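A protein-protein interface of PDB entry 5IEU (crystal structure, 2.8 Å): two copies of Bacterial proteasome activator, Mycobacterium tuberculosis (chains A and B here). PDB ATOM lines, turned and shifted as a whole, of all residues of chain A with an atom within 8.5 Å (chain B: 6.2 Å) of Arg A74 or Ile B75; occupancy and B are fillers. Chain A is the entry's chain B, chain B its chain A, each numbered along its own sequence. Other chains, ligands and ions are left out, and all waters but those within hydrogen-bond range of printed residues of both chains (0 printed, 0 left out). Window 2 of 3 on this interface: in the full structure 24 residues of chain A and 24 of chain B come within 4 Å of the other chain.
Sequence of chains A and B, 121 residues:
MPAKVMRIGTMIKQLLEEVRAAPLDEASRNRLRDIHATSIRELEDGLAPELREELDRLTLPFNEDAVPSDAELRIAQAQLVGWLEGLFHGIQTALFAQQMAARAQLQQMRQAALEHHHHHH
The side-chain amide oxygen of Gln B79 sits close to the backbone carbonyl oxygen of Ala A78.
NH2 of Arg B74 is in salt-bridge range of OD2 of Asp B70.
Among the printed residues, pairs that only touch across the chains: Arg A74 with Ile B75 (3.3 Å), Ile A75 with Arg B74 (3.3 Å), Gln A79 with Ala B78 (3.4 Å), Ala A78 with Ile B75 (3.5 Å), Ile A75 with Ala B78 (3.5 Å), Ile A75 with Ile B75 (3.5 Å), Gly A82 with Gln B79 (3.7 Å), Gln A79 with Gln B79 (3.9 Å) and Val A81 with Gln B79 (3.9 Å).
Arg A74 touches just one residue of chain B: Ile B75 (3.3 Å).
Printed residues of chain B within 4 Å of Ile A75: Arg B74 (3.3 Å), Ile B75 (3.5 Å) and Ala B78 (3.5 Å).
Printed residues of chain B within 4 Å of Gly A82: Gln B79.
No residue of chain A comes within 4 Å of Ala B76.
The nearest printed residue of chain B that does not touch Ile A75 is Ala B71 (5.2 Å).
Of the 22 printed residues of chain A, 6 touch a printed residue of chain B.
Of the 12 printed residues of chain B, 4 touch a printed residue of chain A.
Hydrophobic or aromatic side chains of chain B within 4 Å of the printed part of chain A: Ile B75 and Ala B78.
Among the printed residues, 10 pairs touch across the chains.
Among the printed residues, no Asp or Glu carboxylate lies within 4 Å of a Lys or Arg side-chain nitrogen of the other chain.
Arg A74 touches Ile B75, and with the chains exchanged Ile A75 touches Arg B74.
Ile B75 touches its own counterpart, Ile A75.
Ile A75 touches Ala B78, and with the chains exchanged Ala A78 touches Ile B75.
Gln A79 touches its own counterpart, Gln B79.
Of the 10 pairs that touch across the chains among the printed residues, 8 have their exchanged pair printed and touching as well.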
ATOM      1  N   VAL A  19     -25.072  -3.620   4.936  1.00  0.00           N
ATOM      2  CA  VAL A  19     -24.793  -5.025   4.659  1.00  0.00           C
ATOM      3  C   VAL A  19     -24.722  -5.287   3.159  1.00  0.00           C
ATOM      4  O   VAL A  19     -24.339  -6.376   2.727  1.00  0.00           O
ATOM      5  CB  VAL A  19     -25.858  -5.946   5.282  1.00  0.00           C
ATOM      6  CG1 VAL A  19     -25.467  -6.322   6.703  1.00  0.00           C
ATOM      7  CG2 VAL A  19     -27.222  -5.274   5.256  1.00  0.00           C
ATOM      8  N   ARG A  20     -25.039  -4.285   2.339  1.00  0.00           N
ATOM      9  CA  ARG A  20     -24.875  -4.405   0.878  1.00  0.00           C
ATOM     10  C   ARG A  20     -24.185  -3.311   0.030  1.00  0.00           C
ATOM     11  O   ARG A  20     -24.554  -2.144   0.032  1.00  0.00           O
ATOM     12  CB  ARG A  20     -26.229  -4.592   0.189  1.00  0.00           C
ATOM     13  CG  ARG A  20     -26.202  -5.437  -1.079  1.00  0.00           C
ATOM     14  CD  ARG A  20     -25.180  -4.958  -2.097  1.00  0.00           C
ATOM     15  NE  ARG A  20     -25.735  -4.745  -3.430  1.00  0.00           N
ATOM     16  CZ  ARG A  20     -25.049  -4.896  -4.556  1.00  0.00           C
ATOM     17  NH1 ARG A  20     -23.782  -5.266  -4.522  1.00  0.00           N
ATOM     18  NH2 ARG A  20     -25.633  -4.675  -5.719  1.00  0.00           N
ATOM     19  N   ALA A  21     -23.157  -3.752  -0.689  1.00  0.00           N
ATOM     20  CA  ALA A  21     -22.346  -2.904  -1.553  1.00  0.00           C
ATOM     21  C   ALA A  21     -21.435  -3.864  -2.314  1.00  0.00           C
ATOM     22  O   ALA A  21     -21.219  -4.994  -1.876  1.00  0.00           O
ATOM     23  CB  ALA A  21     -21.676  -1.805  -0.745  1.00  0.00           C
ATOM     24  N   ALA A  22     -20.909  -3.423  -3.452  1.00  0.00           N
ATOM     25  CA  ALA A  22     -19.993  -4.256  -4.223  1.00  0.00           C
ATOM     26  C   ALA A  22     -20.054  -5.710  -3.767  1.00  0.00           C
ATOM     27  O   ALA A  22     -19.416  -6.583  -4.356  1.00  0.00           O
ATOM     28  CB  ALA A  22     -18.573  -3.723  -4.116  1.00  0.00           C
ATOM     29  N   ARG A  29     -11.629  -9.791   3.322  1.00  0.00           N
ATOM     30  CA  ARG A  29     -12.467  -8.600   3.203  1.00  0.00           C
ATOM     31  C   ARG A  29     -12.469  -7.849   4.519  1.00  0.00           C
ATOM     32  O   ARG A  29     -12.877  -8.391   5.543  1.00  0.00           O
ATOM     33  CB  ARG A  29     -13.899  -8.998   2.858  1.00  0.00           C
ATOM     34  CG  ARG A  29     -14.863  -7.837   2.728  1.00  0.00           C
ATOM     35  CD  ARG A  29     -14.396  -6.902   1.647  1.00  0.00           C
ATOM     36  NE  ARG A  29     -15.452  -6.628   0.688  1.00  0.00           N
ATOM     37  CZ  ARG A  29     -15.339  -5.752  -0.307  1.00  0.00           C
ATOM     38  NH1 ARG A  29     -16.376  -5.557  -1.152  1.00  0.00           N
ATOM     39  NH2 ARG A  29     -14.204  -5.045  -0.439  1.00  0.00           N
ATOM     40  N   LEU A  32     -16.399  -6.152   5.719  1.00  0.00           N
ATOM     41  CA  LEU A  32     -17.333  -7.122   6.328  1.00  0.00           C
ATOM     42  C   LEU A  32     -16.890  -7.440   7.720  1.00  0.00           C
ATOM     43  O   LEU A  32     -17.650  -7.346   8.667  1.00  0.00           O
ATOM     44  CB  LEU A  32     -17.414  -8.424   5.524  1.00  0.00           C
ATOM     45  CG  LEU A  32     -18.277  -8.349   4.249  1.00  0.00           C
ATOM     46  CD1 LEU A  32     -18.174  -9.663   3.474  1.00  0.00           C
ATOM     47  CD2 LEU A  32     -19.740  -7.983   4.529  1.00  0.00           C
ATOM     48  N   PRO A  61     -16.387 -16.853   8.633  1.00  0.00           N
ATOM     49  CA  PRO A  61     -15.377 -17.860   8.257  1.00  0.00           C
ATOM     50  C   PRO A  61     -14.518 -17.545   7.026  1.00  0.00           C
ATOM     51  O   PRO A  61     -15.044 -17.525   5.908  1.00  0.00           O
ATOM     52  CB  PRO A  61     -16.254 -19.071   7.954  1.00  0.00           C
ATOM     53  CG  PRO A  61     -17.506 -18.468   7.379  1.00  0.00           C
ATOM     54  CD  PRO A  61     -17.672 -17.093   7.961  1.00  0.00           C
ATOM     55  N   PHE A  62     -13.217 -17.322   7.234  1.00  0.00           N
ATOM     56  CA  PHE A  62     -12.259 -17.135   6.124  1.00  0.00           C
ATOM     57  C   PHE A  62     -11.094 -18.132   6.208  1.00  0.00           C
ATOM     58  O   PHE A  62     -10.759 -18.799   5.220  1.00  0.00           O
ATOM     59  CB  PHE A  62     -11.722 -15.686   6.076  1.00  0.00           C
ATOM     60  CG  PHE A  62     -12.784 -14.634   5.832  1.00  0.00           C
ATOM     61  CD1 PHE A  62     -13.808 -14.852   4.933  1.00  0.00           C
ATOM     62  CD2 PHE A  62     -12.735 -13.413   6.493  1.00  0.00           C
ATOM     63  CE1 PHE A  62     -14.777 -13.896   4.715  1.00  0.00           C
ATOM     64  CE2 PHE A  62     -13.703 -12.445   6.275  1.00  0.00           C
ATOM     65  CZ  PHE A  62     -14.727 -12.689   5.381  1.00  0.00           C
ATOM     66  N   SER A  69     -11.601 -16.087  -1.269  1.00  0.00           N
ATOM     67  CA  SER A  69     -12.296 -16.219  -2.551  1.00  0.00           C
ATOM     68  C   SER A  69     -13.632 -15.551  -2.452  1.00  0.00           C
ATOM     69  O   SER A  69     -14.174 -15.410  -1.365  1.00  0.00           O
ATOM     70  CB  SER A  69     -12.492 -17.687  -2.982  1.00  0.00           C
ATOM     71  OG  SER A  69     -13.685 -18.257  -2.461  1.00  0.00           O
ATOM     72  N   ASP A  70     -14.163 -15.160  -3.601  1.00  0.00           N
ATOM     73  CA  ASP A  70     -15.482 -14.575  -3.661  1.00  0.00           C
ATOM     74  C   ASP A  70     -16.537 -15.472  -2.971  1.00  0.00           C
ATOM     75  O   ASP A  70     -17.347 -14.969  -2.186  1.00  0.00           O
ATOM     76  CB  ASP A  70     -15.870 -14.318  -5.107  1.00  0.00           C
ATOM     77  CG  ASP A  70     -16.913 -13.244  -5.226  1.00  0.00           C
ATOM     78  OD1 ASP A  70     -17.856 -13.224  -4.402  1.00  0.00           O
ATOM     79  OD2 ASP A  70     -16.783 -12.405  -6.137  1.00  0.00           O
ATOM     80  N   ALA A  71     -16.504 -16.785  -3.248  1.00  0.00           N
ATOM     81  CA  ALA A  71     -17.412 -17.793  -2.627  1.00  0.00           C
ATOM     82  C   ALA A  71     -17.591 -17.580  -1.118  1.00  0.00           C
ATOM     83  O   ALA A  71     -18.705 -17.501  -0.604  1.00  0.00           O
ATOM     84  CB  ALA A  71     -16.889 -19.205  -2.886  1.00  0.00           C
ATOM     85  N   GLU A  72     -16.465 -17.463  -0.429  1.00  0.00           N
ATOM     86  CA  GLU A  72     -16.452 -17.268   1.014  1.00  0.00           C
ATOM     87  C   GLU A  72     -16.812 -15.853   1.451  1.00  0.00           C
ATOM     88  O   GLU A  72     -16.943 -15.596   2.650  1.00  0.00           O
ATOM     89  CB  GLU A  72     -15.094 -17.669   1.601  1.00  0.00           C
ATOM     90  CG  GLU A  72     -13.889 -17.410   0.711  1.00  0.00           C
ATOM     91  CD  GLU A  72     -12.721 -18.332   1.013  1.00  0.00           C
ATOM     92  OE1 GLU A  72     -12.569 -18.749   2.179  1.00  0.00           O
ATOM     93  OE2 GLU A  72     -11.936 -18.634   0.086  1.00  0.00           O
ATOM     94  N   LEU A  73     -16.949 -14.952   0.478  1.00  0.00           N
ATOM     95  CA  LEU A  73     -17.350 -13.560   0.704  1.00  0.00           C
ATOM     96  C   LEU A  73     -18.829 -13.393   0.425  1.00  0.00           C
ATOM     97  O   LEU A  73     -19.482 -12.528   0.965  1.00  0.00           O
ATOM     98  CB  LEU A  73     -16.537 -12.595  -0.191  1.00  0.00           C
ATOM     99  CG  LEU A  73     -14.997 -12.577  -0.013  1.00  0.00           C
ATOM    100  CD1 LEU A  73     -14.337 -11.632  -1.016  1.00  0.00           C
ATOM    101  CD2 LEU A  73     -14.538 -12.259   1.418  1.00  0.00           C
ATOM    102  N   ARG A  74     -19.358 -14.215  -0.453  1.00  0.00           N
ATOM    103  CA  ARG A  74     -20.793 -14.268  -0.640  1.00  0.00           C
ATOM    104  C   ARG A  74     -21.359 -14.892   0.630  1.00  0.00           C
ATOM    105  O   ARG A  74     -22.297 -14.382   1.230  1.00  0.00           O
ATOM    106  CB  ARG A  74     -21.144 -15.155  -1.830  1.00  0.00           C
ATOM    107  CG  ARG A  74     -20.295 -14.957  -3.097  1.00  0.00           C
ATOM    108  CD  ARG A  74     -20.926 -13.988  -4.065  1.00  0.00           C
ATOM    109  NE  ARG A  74     -22.357 -14.263  -4.169  1.00  0.00           N
ATOM    110  CZ  ARG A  74     -23.298 -13.352  -4.412  1.00  0.00           C
ATOM    111  NH1 ARG A  74     -22.970 -12.078  -4.598  1.00  0.00           N
ATOM    112  NH2 ARG A  74     -24.575 -13.719  -4.474  1.00  0.00           N
ATOM    113  N   ILE A  75     -20.743 -16.006   1.020  1.00  0.00           N
ATOM    114  CA  ILE A  75     -21.102 -16.773   2.220  1.00  0.00           C
ATOM    115  C   ILE A  75     -20.988 -15.881   3.456  1.00  0.00           C
ATOM    116  O   ILE A  75     -21.988 -15.568   4.077  1.00  0.00           O
ATOM    117  CB  ILE A  75     -20.210 -18.054   2.400  1.00  0.00           C
ATOM    118  CG1 ILE A  75     -20.449 -19.086   1.273  1.00  0.00           C
ATOM    119  CG2 ILE A  75     -20.500 -18.737   3.726  1.00  0.00           C
ATOM    120  CD1 ILE A  75     -19.673 -20.398   1.391  1.00  0.00           C
ATOM    121  N   ALA A  76     -19.773 -15.447   3.795  1.00  0.00           N
ATOM    122  CA  ALA A  76     -19.521 -14.616   5.006  1.00  0.00           C
ATOM    123  C   ALA A  76     -20.488 -13.418   5.159  1.00  0.00           C
ATOM    124  O   ALA A  76     -20.847 -13.034   6.275  1.00  0.00           O
ATOM    125  CB  ALA A  76     -18.075 -14.136   5.037  1.00  0.00           C
ATOM    126  N   GLN A  77     -20.909 -12.851   4.035  1.00  0.00           N
ATOM    127  CA  GLN A  77     -21.813 -11.709   4.022  1.00  0.00           C
ATOM    128  C   GLN A  77     -23.262 -12.110   4.242  1.00  0.00           C
ATOM    129  O   GLN A  77     -24.086 -11.292   4.635  1.00  0.00           O
ATOM    130  CB  GLN A  77     -21.729 -11.038   2.665  1.00  0.00           C
ATOM    131  CG  GLN A  77     -22.727  -9.917   2.445  1.00  0.00           C
ATOM    132  CD  GLN A  77     -23.109  -9.821   1.001  1.00  0.00           C
ATOM    133  OE1 GLN A  77     -22.624 -10.620   0.181  1.00  0.00           O
ATOM    134  NE2 GLN A  77     -24.000  -8.866   0.664  1.00  0.00           N
ATOM    135  N   ALA A  78     -23.607 -13.343   3.910  1.00  0.00           N
ATOM    136  CA  ALA A  78     -24.982 -13.821   4.131  1.00  0.00           C
ATOM    137  C   ALA A  78     -25.121 -14.043   5.619  1.00  0.00           C
ATOM    138  O   ALA A  78     -26.169 -13.733   6.207  1.00  0.00           O
ATOM    139  CB  ALA A  78     -25.242 -15.121   3.383  1.00  0.00           C
ATOM    140  N   GLN A  79     -24.037 -14.562   6.212  1.00  0.00           N
ATOM    141  CA  GLN A  79     -23.967 -14.913   7.634  1.00  0.00           C
ATOM    142  C   GLN A  79     -24.221 -13.709   8.513  1.00  0.00           C
ATOM    143  O   GLN A  79     -24.793 -13.813   9.606  1.00  0.00           O
ATOM    144  CB  GLN A  79     -22.589 -15.470   7.941  1.00  0.00           C
ATOM    145  CG  GLN A  79     -22.422 -16.090   9.333  1.00  0.00           C
ATOM    146  CD  GLN A  79     -21.291 -17.139   9.402  1.00  0.00           C
ATOM    147  OE1 GLN A  79     -20.694 -17.518   8.377  1.00  0.00           O
ATOM    148  NE2 GLN A  79     -21.007 -17.621  10.606  1.00  0.00           N
ATOM    149  N   LEU A  80     -23.836 -12.560   7.990  1.00  0.00           N
ATOM    150  CA  LEU A  80     -23.887 -11.310   8.701  1.00  0.00           C
ATOM    151  C   LEU A  80     -25.199 -10.565   8.552  1.00  0.00           C
ATOM    152  O   LEU A  80     -25.503  -9.666   9.319  1.00  0.00           O
ATOM    153  CB  LEU A  80     -22.745 -10.480   8.163  1.00  0.00           C
ATOM    154  CG  LEU A  80     -22.191  -9.351   9.013  1.00  0.00           C
ATOM    155  CD1 LEU A  80     -20.701  -9.273   8.716  1.00  0.00           C
ATOM    156  CD2 LEU A  80     -22.887  -8.032   8.701  1.00  0.00           C
ATOM    157  N   VAL A  81     -25.974 -10.933   7.553  1.00  0.00           N
ATOM    158  CA  VAL A  81     -27.336 -10.427   7.396  1.00  0.00           C
ATOM    159  C   VAL A  81     -28.290 -11.093   8.402  1.00  0.00           C
ATOM    160  O   VAL A  81     -29.156 -10.452   8.996  1.00  0.00           O
ATOM    161  CB  VAL A  81     -27.883 -10.777   5.989  1.00  0.00           C
ATOM    162  CG1 VAL A  81     -29.314 -10.226   5.807  1.00  0.00           C
ATOM    163  CG2 VAL A  81     -26.903 -10.318   4.884  1.00  0.00           C
ATOM    164  N   GLY A  82     -28.161 -12.412   8.511  1.00  0.00           N
ATOM    165  CA  GLY A  82     -28.946 -13.198   9.456  1.00  0.00           C
ATOM    166  C   GLY A  82     -28.573 -12.879  10.893  1.00  0.00           C
ATOM    167  O   GLY A  82     -29.438 -12.736  11.756  1.00  0.00           O
ATOM    168  N   PRO B  61     -32.331 -16.654   1.224  1.00  0.00           N
ATOM    169  CA  PRO B  61     -32.257 -16.634  -0.208  1.00  0.00           C
ATOM    170  C   PRO B  61     -31.538 -17.855  -0.621  1.00  0.00           C
ATOM    171  O   PRO B  61     -30.378 -17.963  -0.336  1.00  0.00           O
ATOM    172  CB  PRO B  61     -31.355 -15.448  -0.427  1.00  0.00           C
ATOM    173  CG  PRO B  61     -30.430 -15.490   0.753  1.00  0.00           C
ATOM    174  CD  PRO B  61     -31.013 -16.400   1.779  1.00  0.00           C
ATOM    175  N   ASP B  70     -24.988 -26.251  -5.356  1.00  0.00           N
ATOM    176  CA  ASP B  70     -24.310 -26.673  -4.136  1.00  0.00           C
ATOM    177  C   ASP B  70     -23.815 -25.470  -3.340  1.00  0.00           C
ATOM    178  O   ASP B  70     -24.040 -25.377  -2.133  1.00  0.00           O
ATOM    179  CB  ASP B  70     -23.141 -27.601  -4.467  1.00  0.00           C
ATOM    180  CG  ASP B  70     -22.573 -28.285  -3.239  1.00  0.00           C
ATOM    181  OD1 ASP B  70     -23.280 -28.344  -2.210  1.00  0.00           O
ATOM    182  OD2 ASP B  70     -21.421 -28.760  -3.300  1.00  0.00           O
ATOM    183  N   ALA B  71     -23.142 -24.550  -4.023  1.00  0.00           N
ATOM    184  CA  ALA B  71     -22.620 -23.350  -3.382  1.00  0.00           C
ATOM    185  C   ALA B  71     -23.745 -22.520  -2.773  1.00  0.00           C
ATOM    186  O   ALA B  71     -23.598 -21.962  -1.685  1.00  0.00           O
ATOM    187  CB  ALA B  71     -21.825 -22.519  -4.378  1.00  0.00           C
ATOM    188  N   GLU B  72     -24.867 -22.444  -3.480  1.00  0.00           N
ATOM    189  CA  GLU B  72     -26.020 -21.688  -3.009  1.00  0.00           C
ATOM    190  C   GLU B  72     -26.463 -22.166  -1.629  1.00  0.00           C
ATOM    191  O   GLU B  72     -26.915 -21.374  -0.803  1.00  0.00           O
ATOM    192  CB  GLU B  72     -27.179 -21.801  -4.001  1.00  0.00           C
ATOM    193  CG  GLU B  72     -28.436 -21.060  -3.576  1.00  0.00           C
ATOM    194  CD  GLU B  72     -29.702 -21.719  -4.087  1.00  0.00           C
ATOM    195  OE1 GLU B  72     -29.606 -22.573  -4.993  1.00  0.00           O
ATOM    196  OE2 GLU B  72     -30.794 -21.384  -3.582  1.00  0.00           O
ATOM    197  N   LEU B  73     -26.327 -23.466  -1.389  1.00  0.00           N
ATOM    198  CA  LEU B  73     -26.708 -24.052  -0.109  1.00  0.00           C
ATOM    199  C   LEU B  73     -25.807 -23.546   1.013  1.00  0.00           C
ATOM    200  O   LEU B  73     -26.287 -23.128   2.066  1.00  0.00           O
ATOM    201  CB  LEU B  73     -26.654 -25.578  -0.182  1.00  0.00           C
ATOM    202  CG  LEU B  73     -27.999 -26.306  -0.167  1.00  0.00           C
ATOM    203  CD1 LEU B  73     -29.031 -25.545  -0.987  1.00  0.00           C
ATOM    204  CD2 LEU B  73     -27.846 -27.729  -0.680  1.00  0.00           C
ATOM    205  N   ARG B  74     -24.499 -23.592   0.781  1.00  0.00           N
ATOM    206  CA  ARG B  74     -23.529 -23.135   1.770  1.00  0.00           C
ATOM    207  C   ARG B  74     -23.828 -21.706   2.210  1.00  0.00           C
ATOM    208  O   ARG B  74     -23.812 -21.397   3.401  1.00  0.00           O
ATOM    209  CB  ARG B  74     -22.108 -23.229   1.211  1.00  0.00           C
ATOM    210  CG  ARG B  74     -21.027 -23.305   2.275  1.00  0.00           C
ATOM    211  CD  ARG B  74     -19.736 -23.874   1.712  1.00  0.00           C
ATOM    212  NE  ARG B  74     -19.984 -24.850   0.654  1.00  0.00           N
ATOM    213  CZ  ARG B  74     -19.069 -25.248  -0.225  1.00  0.00           C
ATOM    214  NH1 ARG B  74     -17.840 -24.755  -0.175  1.00  0.00           N
ATOM    215  NH2 ARG B  74     -19.383 -26.140  -1.154  1.00  0.00           N
ATOM    216  N   ILE B  75     -24.099 -20.839   1.240  1.00  0.00           N
ATOM    217  CA  ILE B  75     -24.406 -19.442   1.527  1.00  0.00           C
ATOM    218  C   ILE B  75     -25.659 -19.323   2.387  1.00  0.00           C
ATOM    219  O   ILE B  75     -25.696 -18.549   3.343  1.00  0.00           O
ATOM    220  CB  ILE B  75     -24.605 -18.632   0.232  1.00  0.00           C
ATOM    221  CG1 ILE B  75     -23.339 -18.678  -0.626  1.00  0.00           C
ATOM    222  CG2 ILE B  75     -24.982 -17.194   0.557  1.00  0.00           C
ATOM    223  CD1 ILE B  75     -23.303 -17.631  -1.717  1.00  0.00           C
ATOM    224  N   ALA B  76     -26.684 -20.096   2.042  1.00  0.00           N
ATOM    225  CA  ALA B  76     -27.938 -20.084   2.786  1.00  0.00           C
ATOM    226  C   ALA B  76     -27.738 -20.612   4.202  1.00  0.00           C
ATOM    227  O   ALA B  76     -28.301 -20.080   5.158  1.00  0.00           O
ATOM    228  CB  ALA B  76     -28.995 -20.898   2.056  1.00  0.00           C
ATOM    229  N   GLN B  77     -26.934 -21.663   4.329  1.00  0.00           N
ATOM    230  CA  GLN B  77     -26.655 -22.261   5.629  1.00  0.00           C
ATOM    231  C   GLN B  77     -25.965 -21.264   6.554  1.00  0.00           C
ATOM    232  O   GLN B  77     -26.306 -21.158   7.732  1.00  0.00           O
ATOM    233  CB  GLN B  77     -25.790 -23.512   5.467  1.00  0.00           C
ATOM    234  CG  GLN B  77     -25.529 -24.258   6.765  1.00  0.00           C
ATOM    235  CD  GLN B  77     -24.148 -24.882   6.812  1.00  0.00           C
ATOM    236  OE1 GLN B  77     -23.987 -26.080   6.575  1.00  0.00           O
ATOM    237  NE2 GLN B  77     -23.142 -24.072   7.118  1.00  0.00           N
ATOM    238  N   ALA B  78     -24.995 -20.534   6.013  1.00  0.00           N
ATOM    239  CA  ALA B  78     -24.262 -19.541   6.787  1.00  0.00           C
ATOM    240  C   ALA B  78     -25.203 -18.484   7.354  1.00  0.00           C
ATOM    241  O   ALA B  78     -25.062 -18.065   8.503  1.00  0.00           O
ATOM    242  CB  ALA B  78     -23.185 -18.891   5.932  1.00  0.00           C
ATOM    243  N   GLN B  79     -26.165 -18.058   6.542  1.00  0.00           N
ATOM    244  CA  GLN B  79     -27.135 -17.055   6.961  1.00  0.00           C
ATOM    245  C   GLN B  79     -27.994 -17.582   8.106  1.00  0.00           C
ATOM    246  O   GLN B  79     -28.357 -16.837   9.016  1.00  0.00           O
ATOM    247  CB  GLN B  79     -28.021 -16.641   5.786  1.00  0.00           C
ATOM    248  CG  GLN B  79     -29.286 -15.901   6.192  1.00  0.00           C
ATOM    249  CD  GLN B  79     -29.735 -14.897   5.148  1.00  0.00           C
ATOM    250  OE1 GLN B  79     -28.912 -14.254   4.495  1.00  0.00           O
ATOM    251  NE2 GLN B  79     -31.045 -14.761   4.984  1.00  0.00           N
ATOM    252  N   LEU B  80     -28.315 -18.871   8.054  1.00  0.00           N
ATOM    253  CA  LEU B  80     -29.119 -19.504   9.092  1.00  0.00           C
ATOM    254  C   LEU B  80     -28.382 -19.491  10.427  1.00  0.00           C
ATOM    255  O   LEU B  80     -28.975 -19.214  11.471  1.00  0.00           O
ATOM    256  CB  LEU B  80     -29.469 -20.939   8.698  1.00  0.00           C
ATOM    257  CG  LEU B  80     -30.606 -21.599   9.482  1.00  0.00           C
ATOM    258  CD1 LEU B  80     -31.768 -20.631   9.659  1.00  0.00           C
ATOM    259  CD2 LEU B  80     -31.067 -22.874   8.793  1.00  0.00           C
